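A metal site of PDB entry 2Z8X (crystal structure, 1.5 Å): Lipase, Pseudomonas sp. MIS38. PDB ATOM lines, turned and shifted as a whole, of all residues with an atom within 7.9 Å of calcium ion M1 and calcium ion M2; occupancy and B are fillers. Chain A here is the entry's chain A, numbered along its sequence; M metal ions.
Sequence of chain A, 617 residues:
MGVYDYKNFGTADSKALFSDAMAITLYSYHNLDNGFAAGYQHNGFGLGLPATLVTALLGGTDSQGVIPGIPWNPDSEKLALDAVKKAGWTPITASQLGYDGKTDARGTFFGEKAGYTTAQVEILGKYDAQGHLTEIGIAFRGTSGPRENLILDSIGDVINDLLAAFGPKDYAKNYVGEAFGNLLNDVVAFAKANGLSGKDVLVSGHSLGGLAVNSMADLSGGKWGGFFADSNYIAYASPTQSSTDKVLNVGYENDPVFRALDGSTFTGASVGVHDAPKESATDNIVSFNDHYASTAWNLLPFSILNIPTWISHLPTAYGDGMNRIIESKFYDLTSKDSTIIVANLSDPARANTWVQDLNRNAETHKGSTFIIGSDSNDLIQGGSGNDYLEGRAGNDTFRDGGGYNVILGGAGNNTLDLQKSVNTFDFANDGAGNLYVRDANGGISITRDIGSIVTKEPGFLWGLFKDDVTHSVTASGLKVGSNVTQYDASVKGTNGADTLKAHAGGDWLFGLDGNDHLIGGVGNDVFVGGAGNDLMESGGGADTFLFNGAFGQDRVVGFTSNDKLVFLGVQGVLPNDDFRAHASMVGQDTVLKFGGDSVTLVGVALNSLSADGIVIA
Merely in contact with calcium ion M2: Gly 410 (3.9 Å).
Within 4 Å of calcium ion M2: Arg 392, Ala 393, Gly 394, Asp 396, Gly 409, Gly 410, Ala 411 and Asn 414.
The nearest printed residue that does not touch calcium ion M2 is Gly 391 (4.3 Å).
The side-chain carboxylate (OD2) of Asp 396 binds calcium ion M2 (2.3 Å).
The backbone carbonyl oxygen (O) of Gly 394 binds calcium ion M2, 2.3 Å away.
O of Gly 409 is bound to calcium ion M2, at 2.3 Å.
The backbone carbonyl oxygen (O) of Ala 411 is bound to calcium ion M2, 2.4 Å away.
Calcium ion M2 is bound by O of Arg 392.
OD1 of Asn 414 binds calcium ion M2, 2.4 Å away.
N of Gly 391 is in hydrogen-bond range of O of Leu 408, at 2.9 Å.
N of Thr 415 sits at hydrogen-bond distance from O of Asp 396 (2.9 Å).
The backbone NH of Ser 376 lies close to the side-chain hydroxyl of Ser 374 (3.1 Å).
N of Ala 393 sits at hydrogen-bond distance from OD1 of Asp 375.
The guanidinium group of Arg 392 lies within salt-bridge range of the side-chain carboxylate of Asp 375 (3.1 Å).
ND2 of Asn 414 lies within hydrogen-bond range of O of Gly 410 (3.1 Å).
The side-chain amide nitrogen (ND2) of Asn 414 lies within hydrogen-bond range of the backbone carbonyl oxygen (O) of Gly 412, at 3.3 Å.
O of Asp 449 sits at hydrogen-bond distance from ND2 of Asn 414 (2.8 Å).
Within 4 Å of calcium ion M1: Ser 374, Ser 376, Asp 378, Gly 391, Ala 393 and Asp 396.
Calcium ion M1 is bound by O of Gly 391, O of Ser 376, O of Ser 374, O of Ala 393, OD1 of Asp 396 and OD2 of Asp 378.
Slightly farther from calcium ion M1 lies the side-chain carboxylate (OD2) of Asp 396 (3.0 Å).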
ATOM      1  N   ALA A 343     -12.105 -22.060   9.770  1.00  0.00           N
ATOM      2  CA  ALA A 343     -10.753 -21.842  10.299  1.00  0.00           C
ATOM      3  C   ALA A 343     -10.701 -20.469  10.951  1.00  0.00           C
ATOM      4  O   ALA A 343     -10.723 -19.442  10.260  1.00  0.00           O
ATOM      5  CB  ALA A 343      -9.731 -21.951   9.176  1.00  0.00           C
ATOM      6  N   ARG A 350      -2.310 -21.126  13.936  1.00  0.00           N
ATOM      7  CA  ARG A 350      -2.488 -21.501  12.526  1.00  0.00           C
ATOM      8  C   ARG A 350      -1.231 -22.168  11.959  1.00  0.00           C
ATOM      9  O   ARG A 350      -1.323 -23.061  11.103  1.00  0.00           O
ATOM     10  CB  ARG A 350      -2.871 -20.276  11.693  1.00  0.00           C
ATOM     11  CG  ARG A 350      -3.199 -20.594  10.240  1.00  0.00           C
ATOM     12  CD  ARG A 350      -3.565 -19.336   9.456  1.00  0.00           C
ATOM     13  NE  ARG A 350      -2.494 -18.348   9.449  1.00  0.00           N
ATOM     14  CZ  ARG A 350      -2.582 -17.123   9.955  1.00  0.00           C
ATOM     15  NH1 ARG A 350      -3.713 -16.680  10.498  1.00  0.00           N
ATOM     16  NH2 ARG A 350      -1.522 -16.321   9.888  1.00  0.00           N
ATOM     17  N   ILE A 372     -13.574 -24.611   5.751  1.00  0.00           N
ATOM     18  CA  ILE A 372     -13.315 -23.338   5.086  1.00  0.00           C
ATOM     19  C   ILE A 372     -12.075 -22.677   5.685  1.00  0.00           C
ATOM     20  O   ILE A 372     -12.053 -22.324   6.868  1.00  0.00           O
ATOM     21  CB  ILE A 372     -14.527 -22.375   5.187  1.00  0.00           C
ATOM     22  CG1 ILE A 372     -15.852 -23.072   4.826  1.00  0.00           C
ATOM     23  CG2 ILE A 372     -14.307 -21.125   4.333  1.00  0.00           C
ATOM     24  CD1 ILE A 372     -15.877 -23.718   3.441  1.00  0.00           C
ATOM     25  N   GLY A 373     -11.053 -22.515   4.856  1.00  0.00           N
ATOM     26  CA  GLY A 373      -9.797 -21.922   5.292  1.00  0.00           C
ATOM     27  C   GLY A 373      -9.851 -20.404   5.460  1.00  0.00           C
ATOM     28  O   GLY A 373     -10.909 -19.780   5.331  1.00  0.00           O
ATOM     29  N   SER A 374      -8.682 -19.847   5.752  1.00  0.00           N
ATOM     30  CA  SER A 374      -8.489 -18.406   5.880  1.00  0.00           C
ATOM     31  C   SER A 374      -7.704 -17.903   4.676  1.00  0.00           C
ATOM     32  O   SER A 374      -7.226 -18.686   3.856  1.00  0.00           O
ATOM     33  CB  SER A 374      -7.711 -18.100   7.171  1.00  0.00           C
ATOM     34  OG  SER A 374      -6.331 -18.416   7.011  1.00  0.00           O
ATOM     35  N   ASP A 375      -7.551 -16.578   4.574  1.00  0.00           N
ATOM     36  CA  ASP A 375      -6.729 -16.035   3.488  1.00  0.00           C
ATOM     37  C   ASP A 375      -5.221 -16.135   3.737  1.00  0.00           C
ATOM     38  O   ASP A 375      -4.426 -15.667   2.923  1.00  0.00           O
ATOM     39  CB  ASP A 375      -7.175 -14.625   3.138  1.00  0.00           C
ATOM     40  CG  ASP A 375      -8.445 -14.634   2.277  1.00  0.00           C
ATOM     41  OD1 ASP A 375      -8.613 -15.573   1.454  1.00  0.00           O
ATOM     42  OD2 ASP A 375      -9.239 -13.700   2.416  1.00  0.00           O
ATOM     43  N   SER A 376      -4.848 -16.769   4.846  1.00  0.00           N
ATOM     44  CA  SER A 376      -3.439 -17.023   5.145  1.00  0.00           C
ATOM     45  C   SER A 376      -3.093 -18.498   4.942  1.00  0.00           C
ATOM     46  O   SER A 376      -3.947 -19.295   4.475  1.00  0.00           O
ATOM     47  CB  SER A 376      -3.110 -16.543   6.553  1.00  0.00           C
ATOM     48  OG  SER A 376      -3.326 -15.142   6.666  1.00  0.00           O
ATOM     49  N   ASN A 377      -1.854 -18.895   5.257  1.00  0.00           N
ATOM     50  CA  ASN A 377      -1.414 -20.290   5.084  1.00  0.00           C
ATOM     51  C   ASN A 377      -2.065 -21.205   6.103  1.00  0.00           C
ATOM     52  O   ASN A 377      -1.820 -21.071   7.307  1.00  0.00           O
ATOM     53  CB  ASN A 377       0.111 -20.410   5.205  1.00  0.00           C
ATOM     54  CG  ASN A 377       0.861 -19.548   4.203  1.00  0.00           C
ATOM     55  OD1 ASN A 377       0.282 -18.907   3.337  1.00  0.00           O
ATOM     56  ND2 ASN A 377       2.186 -19.549   4.325  1.00  0.00           N
ATOM     57  N   ASP A 378      -2.916 -22.124   5.630  1.00  0.00           N
ATOM     58  CA  ASP A 378      -3.642 -23.030   6.518  1.00  0.00           C
ATOM     59  C   ASP A 378      -3.149 -24.457   6.407  1.00  0.00           C
ATOM     60  O   ASP A 378      -2.655 -24.880   5.355  1.00  0.00           O
ATOM     61  CB  ASP A 378      -5.125 -23.038   6.177  1.00  0.00           C
ATOM     62  CG  ASP A 378      -5.749 -21.672   6.225  1.00  0.00           C
ATOM     63  OD1 ASP A 378      -5.693 -21.022   7.304  1.00  0.00           O
ATOM     64  OD2 ASP A 378      -6.323 -21.254   5.199  1.00  0.00           O
ATOM     65  N   LEU A 379      -3.304 -25.198   7.507  1.00  0.00           N
ATOM     66  CA  LEU A 379      -3.170 -26.643   7.547  1.00  0.00           C
ATOM     67  C   LEU A 379      -4.574 -27.192   7.740  1.00  0.00           C
ATOM     68  O   LEU A 379      -5.211 -26.973   8.779  1.00  0.00           O
ATOM     69  CB  LEU A 379      -2.256 -27.078   8.699  1.00  0.00           C
ATOM     70  CG  LEU A 379      -0.844 -26.484   8.788  1.00  0.00           C
ATOM     71  CD1 LEU A 379      -0.175 -26.987  10.051  1.00  0.00           C
ATOM     72  CD2 LEU A 379       0.006 -26.814   7.556  1.00  0.00           C
ATOM     73  N   ILE A 380      -5.077 -27.884   6.717  1.00  0.00           N
ATOM     74  CA  ILE A 380      -6.465 -28.375   6.718  1.00  0.00           C
ATOM     75  C   ILE A 380      -6.505 -29.896   6.590  1.00  0.00           C
ATOM     76  O   ILE A 380      -5.921 -30.469   5.671  1.00  0.00           O
ATOM     77  CB  ILE A 380      -7.267 -27.739   5.572  1.00  0.00           C
ATOM     78  CG1 ILE A 380      -7.424 -26.224   5.815  1.00  0.00           C
ATOM     79  CG2 ILE A 380      -8.623 -28.419   5.411  1.00  0.00           C
ATOM     80  CD1 ILE A 380      -7.777 -25.402   4.569  1.00  0.00           C
ATOM     81  N   GLU A 390     -11.571 -26.110   1.428  1.00  0.00           N
ATOM     82  CA  GLU A 390     -11.295 -24.892   0.678  1.00  0.00           C
ATOM     83  C   GLU A 390     -10.181 -24.070   1.323  1.00  0.00           C
ATOM     84  O   GLU A 390     -10.323 -23.568   2.428  1.00  0.00           O
ATOM     85  CB  GLU A 390     -12.575 -24.049   0.557  1.00  0.00           C
ATOM     86  CG  GLU A 390     -12.435 -22.876  -0.399  1.00  0.00           C
ATOM     87  CD  GLU A 390     -13.737 -22.089  -0.546  1.00  0.00           C
ATOM     88  OE1 GLU A 390     -14.436 -21.929   0.483  1.00  0.00           O
ATOM     89  OE2 GLU A 390     -14.031 -21.640  -1.677  1.00  0.00           O
ATOM     90  N   GLY A 391      -9.061 -23.937   0.625  1.00  0.00           N
ATOM     91  CA  GLY A 391      -7.906 -23.235   1.192  1.00  0.00           C
ATOM     92  C   GLY A 391      -7.989 -21.713   1.141  1.00  0.00           C
ATOM     93  O   GLY A 391      -7.436 -21.033   2.020  1.00  0.00           O
ATOM     94  N   ARG A 392      -8.658 -21.189   0.125  1.00  0.00           N
ATOM     95  CA  ARG A 392      -8.659 -19.746  -0.155  1.00  0.00           C
ATOM     96  C   ARG A 392      -7.214 -19.270  -0.406  1.00  0.00           C
ATOM     97  O   ARG A 392      -6.360 -20.073  -0.782  1.00  0.00           O
ATOM     98  CB  ARG A 392      -9.336 -18.950   0.985  1.00  0.00           C
ATOM     99  CG  ARG A 392     -10.808 -19.285   1.214  1.00  0.00           C
ATOM    100  CD  ARG A 392     -11.424 -18.430   2.337  1.00  0.00           C
ATOM    101  NE  ARG A 392     -11.247 -16.993   2.112  1.00  0.00           N
ATOM    102  CZ  ARG A 392     -12.163 -16.177   1.579  1.00  0.00           C
ATOM    103  NH1 ARG A 392     -13.337 -16.643   1.187  1.00  0.00           N
ATOM    104  NH2 ARG A 392     -11.887 -14.891   1.436  1.00  0.00           N
ATOM    105  N   ALA A 393      -6.939 -17.984  -0.194  1.00  0.00           N
ATOM    106  CA  ALA A 393      -5.592 -17.454  -0.448  1.00  0.00           C
ATOM    107  C   ALA A 393      -4.597 -18.037   0.546  1.00  0.00           C
ATOM    108  O   ALA A 393      -4.971 -18.707   1.507  1.00  0.00           O
ATOM    109  CB  ALA A 393      -5.585 -15.937  -0.382  1.00  0.00           C
ATOM    110  N   GLY A 394      -3.307 -17.781   0.306  1.00  0.00           N
ATOM    111  CA  GLY A 394      -2.271 -18.369   1.142  1.00  0.00           C
ATOM    112  C   GLY A 394      -1.837 -19.723   0.615  1.00  0.00           C
ATOM    113  O   GLY A 394      -2.548 -20.362  -0.200  1.00  0.00           O
ATOM    114  N   ASN A 395      -0.675 -20.159   1.076  1.00  0.00           N
ATOM    115  CA  ASN A 395      -0.102 -21.445   0.704  1.00  0.00           C
ATOM    116  C   ASN A 395      -0.625 -22.486   1.676  1.00  0.00           C
ATOM    117  O   ASN A 395      -0.168 -22.564   2.817  1.00  0.00           O
ATOM    118  CB  ASN A 395       1.429 -21.398   0.773  1.00  0.00           C
ATOM    119  CG  ASN A 395       2.028 -20.421  -0.230  1.00  0.00           C
ATOM    120  OD1 ASN A 395       1.359 -19.918  -1.139  1.00  0.00           O
ATOM    121  ND2 ASN A 395       3.319 -20.135  -0.053  1.00  0.00           N
ATOM    122  N   ASP A 396      -1.612 -23.255   1.222  1.00  0.00           N
ATOM    123  CA  ASP A 396      -2.307 -24.187   2.109  1.00  0.00           C
ATOM    124  C   ASP A 396      -1.829 -25.614   1.935  1.00  0.00           C
ATOM    125  O   ASP A 396      -1.497 -26.026   0.813  1.00  0.00           O
ATOM    126  CB  ASP A 396      -3.812 -24.100   1.853  1.00  0.00           C
ATOM    127  CG  ASP A 396      -4.326 -22.683   1.958  1.00  0.00           C
ATOM    128  OD1 ASP A 396      -4.176 -22.092   3.048  1.00  0.00           O
ATOM    129  OD2 ASP A 396      -4.870 -22.150   0.965  1.00  0.00           O
ATOM    130  N   THR A 397      -1.787 -26.352   3.039  1.00  0.00           N
ATOM    131  CA  THR A 397      -1.478 -27.770   3.007  1.00  0.00           C
ATOM    132  C   THR A 397      -2.687 -28.567   3.456  1.00  0.00           C
ATOM    133  O   THR A 397      -3.294 -28.263   4.493  1.00  0.00           O
ATOM    134  CB  THR A 397      -0.241 -28.100   3.874  1.00  0.00           C
ATOM    135  OG1 THR A 397       0.838 -27.258   3.466  1.00  0.00           O
ATOM    136  CG2 THR A 397       0.181 -29.563   3.695  1.00  0.00           C
ATOM    137  N   PHE A 398      -3.059 -29.566   2.665  1.00  0.00           N
ATOM    138  CA  PHE A 398      -4.220 -30.392   2.957  1.00  0.00           C
ATOM    139  C   PHE A 398      -3.818 -31.822   3.281  1.00  0.00           C
ATOM    140  O   PHE A 398      -2.879 -32.369   2.664  1.00  0.00           O
ATOM    141  CB  PHE A 398      -5.165 -30.447   1.741  1.00  0.00           C
ATOM    142  CG  PHE A 398      -5.682 -29.103   1.289  1.00  0.00           C
ATOM    143  CD1 PHE A 398      -6.898 -28.602   1.771  1.00  0.00           C
ATOM    144  CD2 PHE A 398      -4.955 -28.336   0.381  1.00  0.00           C
ATOM    145  CE1 PHE A 398      -7.364 -27.354   1.331  1.00  0.00           C
ATOM    146  CE2 PHE A 398      -5.422 -27.105  -0.058  1.00  0.00           C
ATOM    147  CZ  PHE A 398      -6.633 -26.599   0.431  1.00  0.00           C
ATOM    148  N   LEU A 408     -10.015 -27.647  -2.916  1.00  0.00           N
ATOM    149  CA  LEU A 408      -9.750 -26.440  -3.708  1.00  0.00           C
ATOM    150  C   LEU A 408      -8.618 -25.643  -3.084  1.00  0.00           C
ATOM    151  O   LEU A 408      -8.783 -25.024  -2.030  1.00  0.00           O
ATOM    152  CB  LEU A 408     -10.997 -25.558  -3.809  1.00  0.00           C
ATOM    153  CG  LEU A 408     -12.233 -26.180  -4.473  1.00  0.00           C
ATOM    154  CD1 LEU A 408     -13.402 -25.209  -4.437  1.00  0.00           C
ATOM    155  CD2 LEU A 408     -11.929 -26.613  -5.911  1.00  0.00           C
ATOM    156  N   GLY A 409      -7.465 -25.662  -3.740  1.00  0.00           N
ATOM    157  CA  GLY A 409      -6.289 -24.963  -3.230  1.00  0.00           C
ATOM    158  C   GLY A 409      -6.435 -23.458  -3.193  1.00  0.00           C
ATOM    159  O   GLY A 409      -5.796 -22.796  -2.375  1.00  0.00           O
ATOM    160  N   GLY A 410      -7.247 -22.893  -4.096  1.00  0.00           N
ATOM    161  CA  GLY A 410      -7.360 -21.434  -4.237  1.00  0.00           C
ATOM    162  C   GLY A 410      -6.060 -20.794  -4.695  1.00  0.00           C
ATOM    163  O   GLY A 410      -5.176 -21.474  -5.238  1.00  0.00           O
ATOM    164  N   ALA A 411      -5.938 -19.491  -4.463  1.00  0.00           N
ATOM    165  CA  ALA A 411      -4.692 -18.781  -4.792  1.00  0.00           C
ATOM    166  C   ALA A 411      -3.526 -19.368  -3.990  1.00  0.00           C
ATOM    167  O   ALA A 411      -3.738 -20.078  -3.008  1.00  0.00           O
ATOM    168  CB  ALA A 411      -4.841 -17.290  -4.506  1.00  0.00           C
ATOM    169  N   GLY A 412      -2.296 -19.082  -4.419  1.00  0.00           N
ATOM    170  CA  GLY A 412      -1.112 -19.503  -3.676  1.00  0.00           C
ATOM    171  C   GLY A 412      -0.492 -20.789  -4.185  1.00  0.00           C
ATOM    172  O   GLY A 412      -0.957 -21.373  -5.175  1.00  0.00           O
ATOM    173  N   ASN A 413       0.568 -21.231  -3.514  1.00  0.00           N
ATOM    174  CA  ASN A 413       1.202 -22.509  -3.818  1.00  0.00           C
ATOM    175  C   ASN A 413       0.720 -23.517  -2.813  1.00  0.00           C
ATOM    176  O   ASN A 413       1.113 -23.469  -1.642  1.00  0.00           O
ATOM    177  CB  ASN A 413       2.727 -22.375  -3.757  1.00  0.00           C
ATOM    178  CG  ASN A 413       3.268 -21.464  -4.841  1.00  0.00           C
ATOM    179  OD1 ASN A 413       2.897 -21.595  -6.019  1.00  0.00           O
ATOM    180  ND2 ASN A 413       4.151 -20.550  -4.462  1.00  0.00           N
ATOM    181  N   ASN A 414      -0.149 -24.428  -3.249  1.00  0.00           N
ATOM    182  CA  ASN A 414      -0.813 -25.338  -2.343  1.00  0.00           C
ATOM    183  C   ASN A 414      -0.318 -26.777  -2.475  1.00  0.00           C
ATOM    184  O   ASN A 414       0.183 -27.161  -3.535  1.00  0.00           O
ATOM    185  CB  ASN A 414      -2.323 -25.274  -2.577  1.00  0.00           C
ATOM    186  CG  ASN A 414      -2.828 -23.854  -2.628  1.00  0.00           C
ATOM    187  OD1 ASN A 414      -2.873 -23.152  -1.608  1.00  0.00           O
ATOM    188  ND2 ASN A 414      -3.232 -23.410  -3.825  1.00  0.00           N
ATOM    189  N   THR A 415      -0.484 -27.547  -1.403  1.00  0.00           N
ATOM    190  CA  THR A 415       0.062 -28.888  -1.298  1.00  0.00           C
ATOM    191  C   THR A 415      -0.978 -29.875  -0.770  1.00  0.00           C
ATOM    192  O   THR A 415      -1.697 -29.548   0.166  1.00  0.00           O
ATOM    193  CB  THR A 415       1.296 -28.909  -0.344  1.00  0.00           C
ATOM    194  OG1 THR A 415       2.281 -28.005  -0.854  1.00  0.00           O
ATOM    195  CG2 THR A 415       1.892 -30.317  -0.219  1.00  0.00           C
ATOM    196  N   ASP A 449      -5.955 -26.411  -8.297  1.00  0.00           N
ATOM    197  CA  ASP A 449      -4.969 -25.472  -7.774  1.00  0.00           C
ATOM    198  C   ASP A 449      -4.074 -26.070  -6.697  1.00  0.00           C
ATOM    199  O   ASP A 449      -3.593 -25.367  -5.801  1.00  0.00           O
ATOM    200  CB  ASP A 449      -5.648 -24.177  -7.291  1.00  0.00           C
ATOM    201  CG  ASP A 449      -6.397 -23.480  -8.391  1.00  0.00           C
ATOM    202  OD1 ASP A 449      -5.766 -23.154  -9.430  1.00  0.00           O
ATOM    203  OD2 ASP A 449      -7.618 -23.285  -8.244  1.00  0.00           O
ATOM    204  N   ILE A 450      -3.837 -27.368  -6.791  1.00  0.00           N
ATOM    205  CA  ILE A 450      -2.836 -28.000  -5.938  1.00  0.00           C
ATOM    206  C   ILE A 450      -1.680 -28.428  -6.837  1.00  0.00           C
ATOM    207  O   ILE A 450      -1.828 -29.327  -7.661  1.00  0.00           O
ATOM    208  CB  ILE A 450      -3.457 -29.122  -5.081  1.00  0.00           C
ATOM    209  CG1 ILE A 450      -4.394 -28.482  -4.025  1.00  0.00           C
ATOM    210  CG2 ILE A 450      -2.368 -29.954  -4.406  1.00  0.00           C
ATOM    211  CD1 ILE A 450      -5.379 -29.408  -3.394  1.00  0.00           C
HETATM  212 CA    CA M   1      -5.619 -20.214   3.170  1.00  0.00          CA
HETATM  213 CA    CA M   2      -4.422 -21.354  -1.155  1.00  0.00          CA
